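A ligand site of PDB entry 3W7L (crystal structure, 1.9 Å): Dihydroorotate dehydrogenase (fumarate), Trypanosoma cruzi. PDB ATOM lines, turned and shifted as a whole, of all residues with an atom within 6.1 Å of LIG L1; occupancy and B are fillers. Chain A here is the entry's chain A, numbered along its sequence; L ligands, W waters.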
ATOM      1  N   ALA A  20      -0.470  -0.283  17.788  1.00  0.00           N
ATOM      2  CA  ALA A  20      -0.357   1.021  17.260  1.00  0.00           C
ATOM      3  C   ALA A  20       1.047   1.542  17.444  1.00  0.00           C
ATOM      4  O   ALA A  20       1.670   1.382  18.498  1.00  0.00           O
ATOM      5  CB  ALA A  20      -1.328   2.007  17.930  1.00  0.00           C
ATOM      6  N   LYS A  44      -1.112   4.086  12.627  1.00  0.00           N
ATOM      7  CA  LYS A  44      -0.426   4.881  13.576  1.00  0.00           C
ATOM      8  C   LYS A  44      -1.329   5.921  14.196  1.00  0.00           C
ATOM      9  O   LYS A  44      -2.016   6.656  13.472  1.00  0.00           O
ATOM     10  CB  LYS A  44       0.733   5.584  12.914  1.00  0.00           C
ATOM     11  CG  LYS A  44       1.555   6.534  13.787  1.00  0.00           C
ATOM     12  CD  LYS A  44       2.307   5.966  14.941  1.00  0.00           C
ATOM     13  CE  LYS A  44       2.952   7.096  15.803  1.00  0.00           C
ATOM     14  NZ  LYS A  44       3.528   6.858  17.225  1.00  0.00           N
ATOM     15  N   SER A  45      -1.258   6.028  15.523  1.00  0.00           N
ATOM     16  CA  SER A  45      -2.024   7.025  16.285  1.00  0.00           C
ATOM     17  C   SER A  45      -1.728   8.401  15.670  1.00  0.00           C
ATOM     18  O   SER A  45      -0.560   8.747  15.461  1.00  0.00           O
ATOM     19  CB  SER A  45      -1.696   7.083  17.740  1.00  0.00           C
ATOM     20  OG  SER A  45      -2.146   5.917  18.350  1.00  0.00           O
ATOM     21  N   ARG A  51       3.099  15.379  12.201  1.00  0.00           N
ATOM     22  CA  ARG A  51       4.134  15.590  13.184  1.00  0.00           C
ATOM     23  C   ARG A  51       5.424  14.860  12.857  1.00  0.00           C
ATOM     24  O   ARG A  51       5.397  13.721  12.462  1.00  0.00           O
ATOM     25  CB  ARG A  51       3.733  15.152  14.603  1.00  0.00           C
ATOM     26  CG  ARG A  51       2.584  15.916  15.302  1.00  0.00           C
ATOM     27  CD  ARG A  51       2.239  15.186  16.589  1.00  0.00           C
ATOM     28  NE  ARG A  51       3.285  15.118  17.612  1.00  0.00           N
ATOM     29  CZ  ARG A  51       3.578  16.091  18.450  1.00  0.00           C
ATOM     30  NH1 ARG A  51       2.927  17.290  18.371  1.00  0.00           N
ATOM     31  NH2 ARG A  51       4.526  15.902  19.304  1.00  0.00           N
ATOM     32  N   ASN A  54       9.805  13.512  17.987  1.00  0.00           N
ATOM     33  CA  ASN A  54      10.999  13.918  18.774  1.00  0.00           C
ATOM     34  C   ASN A  54      12.314  13.693  18.037  1.00  0.00           C
ATOM     35  O   ASN A  54      12.404  12.902  17.065  1.00  0.00           O
ATOM     36  CB  ASN A  54      11.028  13.149  20.063  1.00  0.00           C
ATOM     37  CG  ASN A  54      10.073  13.653  21.110  1.00  0.00           C
ATOM     38  OD1 ASN A  54       9.644  14.833  21.102  1.00  0.00           O
ATOM     39  ND2 ASN A  54       9.712  12.793  22.004  1.00  0.00           N
ATOM     40  N   ASN A  68      10.930   3.845  24.238  1.00  0.00           N
ATOM     41  CA  ASN A  68      10.664   4.814  23.179  1.00  0.00           C
ATOM     42  C   ASN A  68      10.111   6.129  23.759  1.00  0.00           C
ATOM     43  O   ASN A  68       9.309   6.144  24.694  1.00  0.00           O
ATOM     44  CB  ASN A  68       9.729   4.282  22.056  1.00  0.00           C
ATOM     45  CG  ASN A  68       8.263   4.488  22.374  1.00  0.00           C
ATOM     46  OD1 ASN A  68       7.708   5.609  22.197  1.00  0.00           O
ATOM     47  ND2 ASN A  68       7.612   3.469  22.867  1.00  0.00           N
ATOM     48  N   SER A  69      10.519   7.227  23.156  1.00  0.00           N
ATOM     49  CA  SER A  69       9.847   8.512  23.335  1.00  0.00           C
ATOM     50  C   SER A  69       9.759   9.143  21.973  1.00  0.00           C
ATOM     51  O   SER A  69      10.464  10.101  21.654  1.00  0.00           O
ATOM     52  CB  SER A  69      10.549   9.426  24.351  1.00  0.00           C
ATOM     53  OG  SER A  69      10.448   8.971  25.666  1.00  0.00           O
ATOM     54  N   MET A  70       8.865   8.577  21.166  1.00  0.00           N
ATOM     55  CA  MET A  70       8.810   8.920  19.735  1.00  0.00           C
ATOM     56  C   MET A  70       8.301  10.345  19.535  1.00  0.00           C
ATOM     57  O   MET A  70       8.665  11.041  18.556  1.00  0.00           O
ATOM     58  CB  MET A  70       7.854   8.007  19.033  1.00  0.00           C
ATOM     59  CG  MET A  70       8.220   6.564  19.013  1.00  0.00           C
ATOM     60  SD  MET A  70       9.798   6.133  18.312  1.00  0.00           S
ATOM     61  CE  MET A  70       9.559   6.426  16.629  1.00  0.00           C
ATOM     62  N   GLY A  71       7.438  10.808  20.432  1.00  0.00           N
ATOM     63  CA  GLY A  71       6.853  12.141  20.260  1.00  0.00           C
ATOM     64  C   GLY A  71       5.713  12.177  19.256  1.00  0.00           C
ATOM     65  O   GLY A  71       5.427  13.245  18.671  1.00  0.00           O
ATOM     66  N   LEU A  72       5.060  11.046  19.048  1.00  0.00           N
ATOM     67  CA  LEU A  72       3.906  10.924  18.135  1.00  0.00           C
ATOM     68  C   LEU A  72       4.148  11.428  16.712  1.00  0.00           C
ATOM     69  O   LEU A  72       3.326  12.169  16.160  1.00  0.00           O
ATOM     70  CB  LEU A  72       2.690  11.699  18.654  1.00  0.00           C
ATOM     71  CG  LEU A  72       1.364  10.994  18.892  1.00  0.00           C
ATOM     72  CD1 LEU A  72       0.275  11.943  19.389  1.00  0.00           C
ATOM     73  CD2 LEU A  72       0.950   9.943  17.926  1.00  0.00           C
ATOM     74  N   PRO A  73       5.189  10.953  16.093  1.00  0.00           N
ATOM     75  CA  PRO A  73       5.370  11.278  14.644  1.00  0.00           C
ATOM     76  C   PRO A  73       4.259  10.615  13.862  1.00  0.00           C
ATOM     77  O   PRO A  73       3.956   9.474  14.126  1.00  0.00           O
ATOM     78  CB  PRO A  73       6.724  10.646  14.315  1.00  0.00           C
ATOM     79  CG  PRO A  73       6.891   9.452  15.267  1.00  0.00           C
ATOM     80  CD  PRO A  73       6.100   9.866  16.535  1.00  0.00           C
ATOM     81  N   SER A 100      -4.974   9.968  18.476  1.00  0.00           N
ATOM     82  CA  SER A 100      -4.388  10.402  19.709  1.00  0.00           C
ATOM     83  C   SER A 100      -4.198  11.901  19.789  1.00  0.00           C
ATOM     84  O   SER A 100      -3.072  12.416  19.887  1.00  0.00           O
ATOM     85  CB  SER A 100      -3.040   9.655  19.856  1.00  0.00           C
ATOM     86  OG  SER A 100      -2.557   9.847  21.170  1.00  0.00           O
ATOM     87  N   LEU A 102      -4.088  15.810  21.051  1.00  0.00           N
ATOM     88  CA  LEU A 102      -3.346  16.378  22.144  1.00  0.00           C
ATOM     89  C   LEU A 102      -4.277  17.193  23.069  1.00  0.00           C
ATOM     90  O   LEU A 102      -3.797  17.739  24.081  1.00  0.00           O
ATOM     91  CB  LEU A 102      -2.205  17.283  21.634  1.00  0.00           C
ATOM     92  CG  LEU A 102      -1.215  16.593  20.647  1.00  0.00           C
ATOM     93  CD1 LEU A 102      -0.059  17.493  20.277  1.00  0.00           C
ATOM     94  CD2 LEU A 102      -0.702  15.298  21.222  1.00  0.00           C
ATOM     95  N   ASN A 128      -6.624   6.566  21.758  1.00  0.00           N
ATOM     96  CA  ASN A 128      -5.495   6.428  22.644  1.00  0.00           C
ATOM     97  C   ASN A 128      -5.564   7.394  23.801  1.00  0.00           C
ATOM     98  O   ASN A 128      -5.372   8.554  23.619  1.00  0.00           O
ATOM     99  CB  ASN A 128      -4.169   6.664  21.908  1.00  0.00           C
ATOM    100  CG  ASN A 128      -2.964   6.526  22.782  1.00  0.00           C
ATOM    101  OD1 ASN A 128      -3.045   6.010  23.792  1.00  0.00           O
ATOM    102  ND2 ASN A 128      -1.846   6.911  22.285  1.00  0.00           N
ATOM    103  N   SER A 130      -3.580   6.952  26.601  1.00  0.00           N
ATOM    104  CA  SER A 130      -2.313   6.834  27.242  1.00  0.00           C
ATOM    105  C   SER A 130      -1.501   7.911  26.627  1.00  0.00           C
ATOM    106  O   SER A 130      -0.451   7.669  26.143  1.00  0.00           O
ATOM    107  CB  SER A 130      -1.680   5.438  27.021  1.00  0.00           C
ATOM    108  OG  SER A 130      -2.564   4.493  26.416  1.00  0.00           O
ATOM    109  N   CYS A 131      -2.031   9.104  26.673  1.00  0.00           N
ATOM    110  CA  CYS A 131      -1.547  10.242  25.983  1.00  0.00           C
ATOM    111  C   CYS A 131      -1.490  11.566  26.823  1.00  0.00           C
ATOM    112  O   CYS A 131      -2.269  11.808  27.687  1.00  0.00           O
ATOM    113  CB  CYS A 131      -2.396  10.469  24.733  1.00  0.00           C
ATOM    114  SG  CYS A 131      -3.950  11.372  24.872  1.00  0.00           S
ATOM    115  N   PRO A 132      -0.422  12.398  26.469  1.00  0.00           N
ATOM    116  CA  PRO A 132      -0.402  13.697  27.163  1.00  0.00           C
ATOM    117  C   PRO A 132      -1.591  14.614  26.921  1.00  0.00           C
ATOM    118  O   PRO A 132      -2.206  14.595  25.924  1.00  0.00           O
ATOM    119  CB  PRO A 132       0.843  14.398  26.616  1.00  0.00           C
ATOM    120  CG  PRO A 132       1.135  13.768  25.339  1.00  0.00           C
ATOM    121  CD  PRO A 132       0.848  12.355  25.582  1.00  0.00           C
ATOM    122  N   LYS A 165      -7.407   2.640  24.050  1.00  0.00           N
ATOM    123  CA  LYS A 165      -6.069   2.092  24.391  1.00  0.00           C
ATOM    124  C   LYS A 165      -5.678   2.688  25.700  1.00  0.00           C
ATOM    125  O   LYS A 165      -5.646   3.944  25.882  1.00  0.00           O
ATOM    126  CB  LYS A 165      -5.076   2.447  23.326  1.00  0.00           C
ATOM    127  CG  LYS A 165      -3.630   2.064  23.659  1.00  0.00           C
ATOM    128  CD  LYS A 165      -3.442   0.639  23.322  1.00  0.00           C
ATOM    129  CE  LYS A 165      -1.971   0.300  23.318  1.00  0.00           C
ATOM    130  NZ  LYS A 165      -1.270   0.629  22.074  1.00  0.00           N
ATOM    131  N   ASN A 195      -0.772   0.049  26.771  1.00  0.00           N
ATOM    132  CA  ASN A 195       0.238   0.911  26.214  1.00  0.00           C
ATOM    133  C   ASN A 195       1.536   0.682  27.034  1.00  0.00           C
ATOM    134  O   ASN A 195       1.548  -0.086  27.946  1.00  0.00           O
ATOM    135  CB  ASN A 195      -0.233   2.385  26.195  1.00  0.00           C
ATOM    136  CG  ASN A 195       0.340   3.171  25.032  1.00  0.00           C
ATOM    137  OD1 ASN A 195       1.474   3.120  24.799  1.00  0.00           O
ATOM    138  ND2 ASN A 195      -0.509   3.834  24.265  1.00  0.00           N
ATOM    139  N   SER A 196       2.602   1.366  26.662  1.00  0.00           N
ATOM    140  CA  SER A 196       3.874   1.138  27.307  1.00  0.00           C
ATOM    141  C   SER A 196       3.857   1.442  28.811  1.00  0.00           C
ATOM    142  O   SER A 196       3.043   2.192  29.272  1.00  0.00           O
ATOM    143  CB  SER A 196       5.014   1.868  26.620  1.00  0.00           C
ATOM    144  OG  SER A 196       4.600   2.982  25.984  1.00  0.00           O
ATOM    145  N   LYS A 215      13.629  13.681  26.725  1.00  0.00           N
ATOM    146  CA  LYS A 215      13.278  13.491  28.129  1.00  0.00           C
ATOM    147  C   LYS A 215      14.444  12.905  28.961  1.00  0.00           C
ATOM    148  O   LYS A 215      14.253  12.139  29.892  1.00  0.00           O
ATOM    149  CB  LYS A 215      12.053  12.568  28.219  1.00  0.00           C
ATOM    150  CG  LYS A 215      10.741  13.178  27.721  1.00  0.00           C
ATOM    151  CD  LYS A 215       9.701  12.057  27.440  1.00  0.00           C
ATOM    152  CE  LYS A 215       9.172  11.520  28.682  1.00  0.00           C
ATOM    153  NZ  LYS A 215       7.916  10.757  28.581  1.00  0.00           N
ATOM    154  N   GLY A 220       8.863   5.102  27.267  1.00  0.00           N
ATOM    155  CA  GLY A 220       7.926   4.031  27.536  1.00  0.00           C
ATOM    156  C   GLY A 220       8.576   2.688  27.244  1.00  0.00           C
ATOM    157  O   GLY A 220       9.221   2.510  26.259  1.00  0.00           O
HETATM  158  O1  LIG L   1       4.720   8.644  20.360  1.00  0.00           O
HETATM  159  C1  LIG L   1       4.964   8.135  21.448  1.00  0.00           C
HETATM  160  O2  LIG L   1       5.910   8.496  22.112  1.00  0.00           O
HETATM  161  C2  LIG L   1       4.119   7.063  21.998  1.00  0.00           C
HETATM  162  N1  LIG L   1       4.827   5.964  22.432  1.00  0.00           N
HETATM  163  C3  LIG L   1       4.185   4.845  23.022  1.00  0.00           C
HETATM  164  O3  LIG L   1       4.811   3.880  23.471  1.00  0.00           O
HETATM  165  N2  LIG L   1       2.851   4.949  23.208  1.00  0.00           N
HETATM  166  C4  LIG L   1       2.102   6.108  22.810  1.00  0.00           C
HETATM  167  O4  LIG L   1       0.872   6.072  23.027  1.00  0.00           O
HETATM  168  C5  LIG L   1       2.786   7.197  22.183  1.00  0.00           C
HETATM  169  C6  LIG L   1       2.133   8.408  21.839  1.00  0.00           C
HETATM  170  C7  LIG L   1       1.601   9.122  23.136  1.00  0.00           C
HETATM  171  C8  LIG L   1       2.624   9.756  23.858  1.00  0.00           C
HETATM  172  C9  LIG L   1       3.278   9.110  24.975  1.00  0.00           C
HETATM  173  C10 LIG L   1       4.359   9.678  25.677  1.00  0.00           C
HETATM  174  C11 LIG L   1       4.863  10.920  25.249  1.00  0.00           C
HETATM  175  C12 LIG L   1       4.251  11.598  24.163  1.00  0.00           C
HETATM  176  C13 LIG L   1       4.776  12.820  23.753  1.00  0.00           C
HETATM  177  C14 LIG L   1       3.176  11.044  23.446  1.00  0.00           C
HETATM  178  C15 LIG L   1       2.622  11.777  22.375  1.00  0.00           C
HETATM  179  C16 LIG L   1       3.103  13.057  22.025  1.00  0.00           C
HETATM  180  C17 LIG L   1       4.179  13.540  22.694  1.00  0.00           C
HETATM  181  O5  LIG L   1       4.696  14.782  22.284  1.00  0.00           O
HETATM  182  C18 LIG L   1       5.958  15.167  22.818  1.00  0.00           C
HETATM  183  N1  LG2 L   2       0.722   3.066  21.300  1.00  0.00           N
HETATM  184  C1  LG2 L   2      -0.289   3.821  20.796  1.00  0.00           C
HETATM  185  O1  LG2 L   2      -1.433   3.620  21.222  1.00  0.00           O
HETATM  186  N2  LG2 L   2      -0.074   4.787  19.895  1.00  0.00           N
HETATM  187  C2  LG2 L   2       1.109   5.026  19.326  1.00  0.00           C
HETATM  188  O2  LG2 L   2       1.348   5.842  18.373  1.00  0.00           O
HETATM  189  C3  LG2 L   2       2.204   4.207  19.739  1.00  0.00           C
HETATM  190  N3  LG2 L   2       3.429   4.410  19.224  1.00  0.00           N
HETATM  191  C4  LG2 L   2       4.431   3.536  19.512  1.00  0.00           C
HETATM  192  C5  LG2 L   2       5.676   3.593  18.880  1.00  0.00           C
HETATM  193  C6  LG2 L   2       6.713   2.695  19.188  1.00  0.00           C
HETATM  194  C7  LG2 L   2       8.032   2.828  18.555  1.00  0.00           C
HETATM  195  C8  LG2 L   2       6.490   1.655  20.161  1.00  0.00           C
HETATM  196  C9  LG2 L   2       7.562   0.689  20.549  1.00  0.00           C
HETATM  197  C10 LG2 L   2       5.246   1.575  20.788  1.00  0.00           C
HETATM  198  C11 LG2 L   2       4.199   2.463  20.480  1.00  0.00           C
HETATM  199  N4  LG2 L   2       2.982   2.409  21.126  1.00  0.00           N
HETATM  200  C12 LG2 L   2       1.950   3.222  20.773  1.00  0.00           C
HETATM  201  C13 LG2 L   2       2.757   1.394  22.105  1.00  0.00           C
HETATM  202  C14 LG2 L   2       2.511   0.046  21.542  1.00  0.00           C
HETATM  203  O3  LG2 L   2       1.306   0.051  20.814  1.00  0.00           O
HETATM  204  C15 LG2 L   2       2.335  -0.974  22.686  1.00  0.00           C
HETATM  205  O4  LG2 L   2       1.155  -0.582  23.481  1.00  0.00           O
HETATM  206  C16 LG2 L   2       3.549  -1.123  23.623  1.00  0.00           C
HETATM  207  O5  LG2 L   2       4.764  -1.083  22.814  1.00  0.00           O
HETATM  208  C17 LG2 L   2       3.513  -2.503  24.337  1.00  0.00           C
HETATM  209  O6  LG2 L   2       3.486  -3.637  23.506  1.00  0.00           O
HETATM  210  P1  LG2 L   2       4.815  -4.536  23.241  1.00  0.00           P
HETATM  211  O7  LG2 L   2       4.369  -5.522  22.209  1.00  0.00           O
HETATM  212  O8  LG2 L   2       5.283  -4.968  24.565  1.00  0.00           O
HETATM  213  O9  LG2 L   2       5.797  -3.510  22.677  1.00  0.00           O
HETATM  214  O   HOH W   1       1.953   6.177  26.258  1.00  0.00           O
HETATM  215  O   HOH W   2       6.588   7.203  24.841  1.00  0.00           O
HETATM  216  O   HOH W   3       4.422   5.592  25.856  1.00  0.00           O
HETATM  217  O   HOH W   4       7.594  10.733  23.546  1.00  0.00           O
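An oxygen (O2) of LIG L1 sits at hydrogen-bond distance from the backbone NH of Met 70 (3.1 Å).
The guanidinium group (NH2) of Arg 51 is in hydrogen-bond range of an oxygen (O5) of LIG L1 (3.2 Å).
An oxygen (O3) of LG2 L2 lies within hydrogen-bond range of the backbone carbonyl oxygen of Ala 20, 2.7 Å away.
The side-chain hydroxyl (OG) of Ser 196 lies within hydrogen-bond range of an oxygen (O3) of LIG L1, 2.7 Å away.
NZ of Lys 44 is in salt-bridge range of O1 of LIG L1 (3.8 Å).
The side-chain amino group (NZ) of Lys 44 is in hydrogen-bond range of an oxygen (O2) of LG2 L2, 2.7 Å away.
An oxygen (O3) of LIG L1 is in hydrogen-bond range of the side-chain amide nitrogen (ND2) of Asn 68 (2.9 Å).
The side-chain amide oxygen (OD1) of Asn 195 lies within hydrogen-bond range of a nitrogen (N2) of LIG L1, at 2.8 Å.
The backbone NH (N) of Gly 71 sits at hydrogen-bond distance from an oxygen (O2) of LIG L1.
NZ of Lys 165 sits at hydrogen-bond distance from O3 of LG2 L2 (2.9 Å).
A nitrogen (N2) of LG2 L2 sits at hydrogen-bond distance from the side-chain hydroxyl of Ser 45, at 2.8 Å.
The side-chain amide nitrogen (ND2) of Asn 195 sits at hydrogen-bond distance from an oxygen (O1) of LG2 L2 (3.2 Å).
The side-chain amide nitrogen (ND2) of Asn 128 is in hydrogen-bond range of an oxygen (O1) of LG2 L2 (3.5 Å).
The backbone NH of Leu 72 is in hydrogen-bond range of an oxygen (O1) of LIG L1 (2.8 Å).
ND2 of Asn 128 lies within hydrogen-bond range of O4 of LIG L1, at 2.9 Å.
N2 of LIG L1 sits close to N1 of LG2 L2, at 3.4 Å.
The backbone carbonyl oxygen (O) of Gly 71 sits at hydrogen-bond distance from the guanidinium group (NH2) of Arg 51, 2.9 Å away.
The backbone carbonyl oxygen (O) of Asn 68 is in hydrogen-bond range of the backbone NH (N) of Gly 220, 2.8 Å away.
The side-chain hydroxyl (OG) of Ser 130 lies within hydrogen-bond range of the backbone carbonyl oxygen (O) of Lys 165, at 3.2 Å.
The side-chain amide nitrogen (ND2) of Asn 54 lies within hydrogen-bond range of the backbone carbonyl oxygen (O) of Ser 69 (2.8 Å).
The side-chain amide nitrogen (ND2) of Asn 195 is in hydrogen-bond range of the side-chain hydroxyl (OG) of Ser 130.
The backbone NH of Ser 130 is in hydrogen-bond range of the side-chain amide oxygen of Asn 128 (3.0 Å).
O of Leu 72 lies close to NE of Arg 51, 3.3 Å away.
O of Asn 128 sits at hydrogen-bond distance from SG of Cys 131 (3.4 Å).
C of Ser 69 touches O2 of LIG L1 (3.9 Å).
Ser 130 touches LIG L1.
Pro 132 touches LIG L1 (CD to C14, 3.4 Å).
Hydrophobic or aromatic side chains that line LIG L1: Met 70, Leu 72 and Pro 132.
Water W3 bridges OG of Ser 196 (2.6 Å) and O3 of LIG L1 (3.0 Å).
Water W2 bridges the backbone carbonyl oxygen (O) of Asn 68 (2.9 Å) and an oxygen (O2) of LIG L1 (3.1 Å).
Water W1 lies within hydrogen-bond range of O of Ser 130 (2.8 Å), N2 of LIG L1 (3.4 Å) and OD1 of Asn 195 (3.4 Å).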
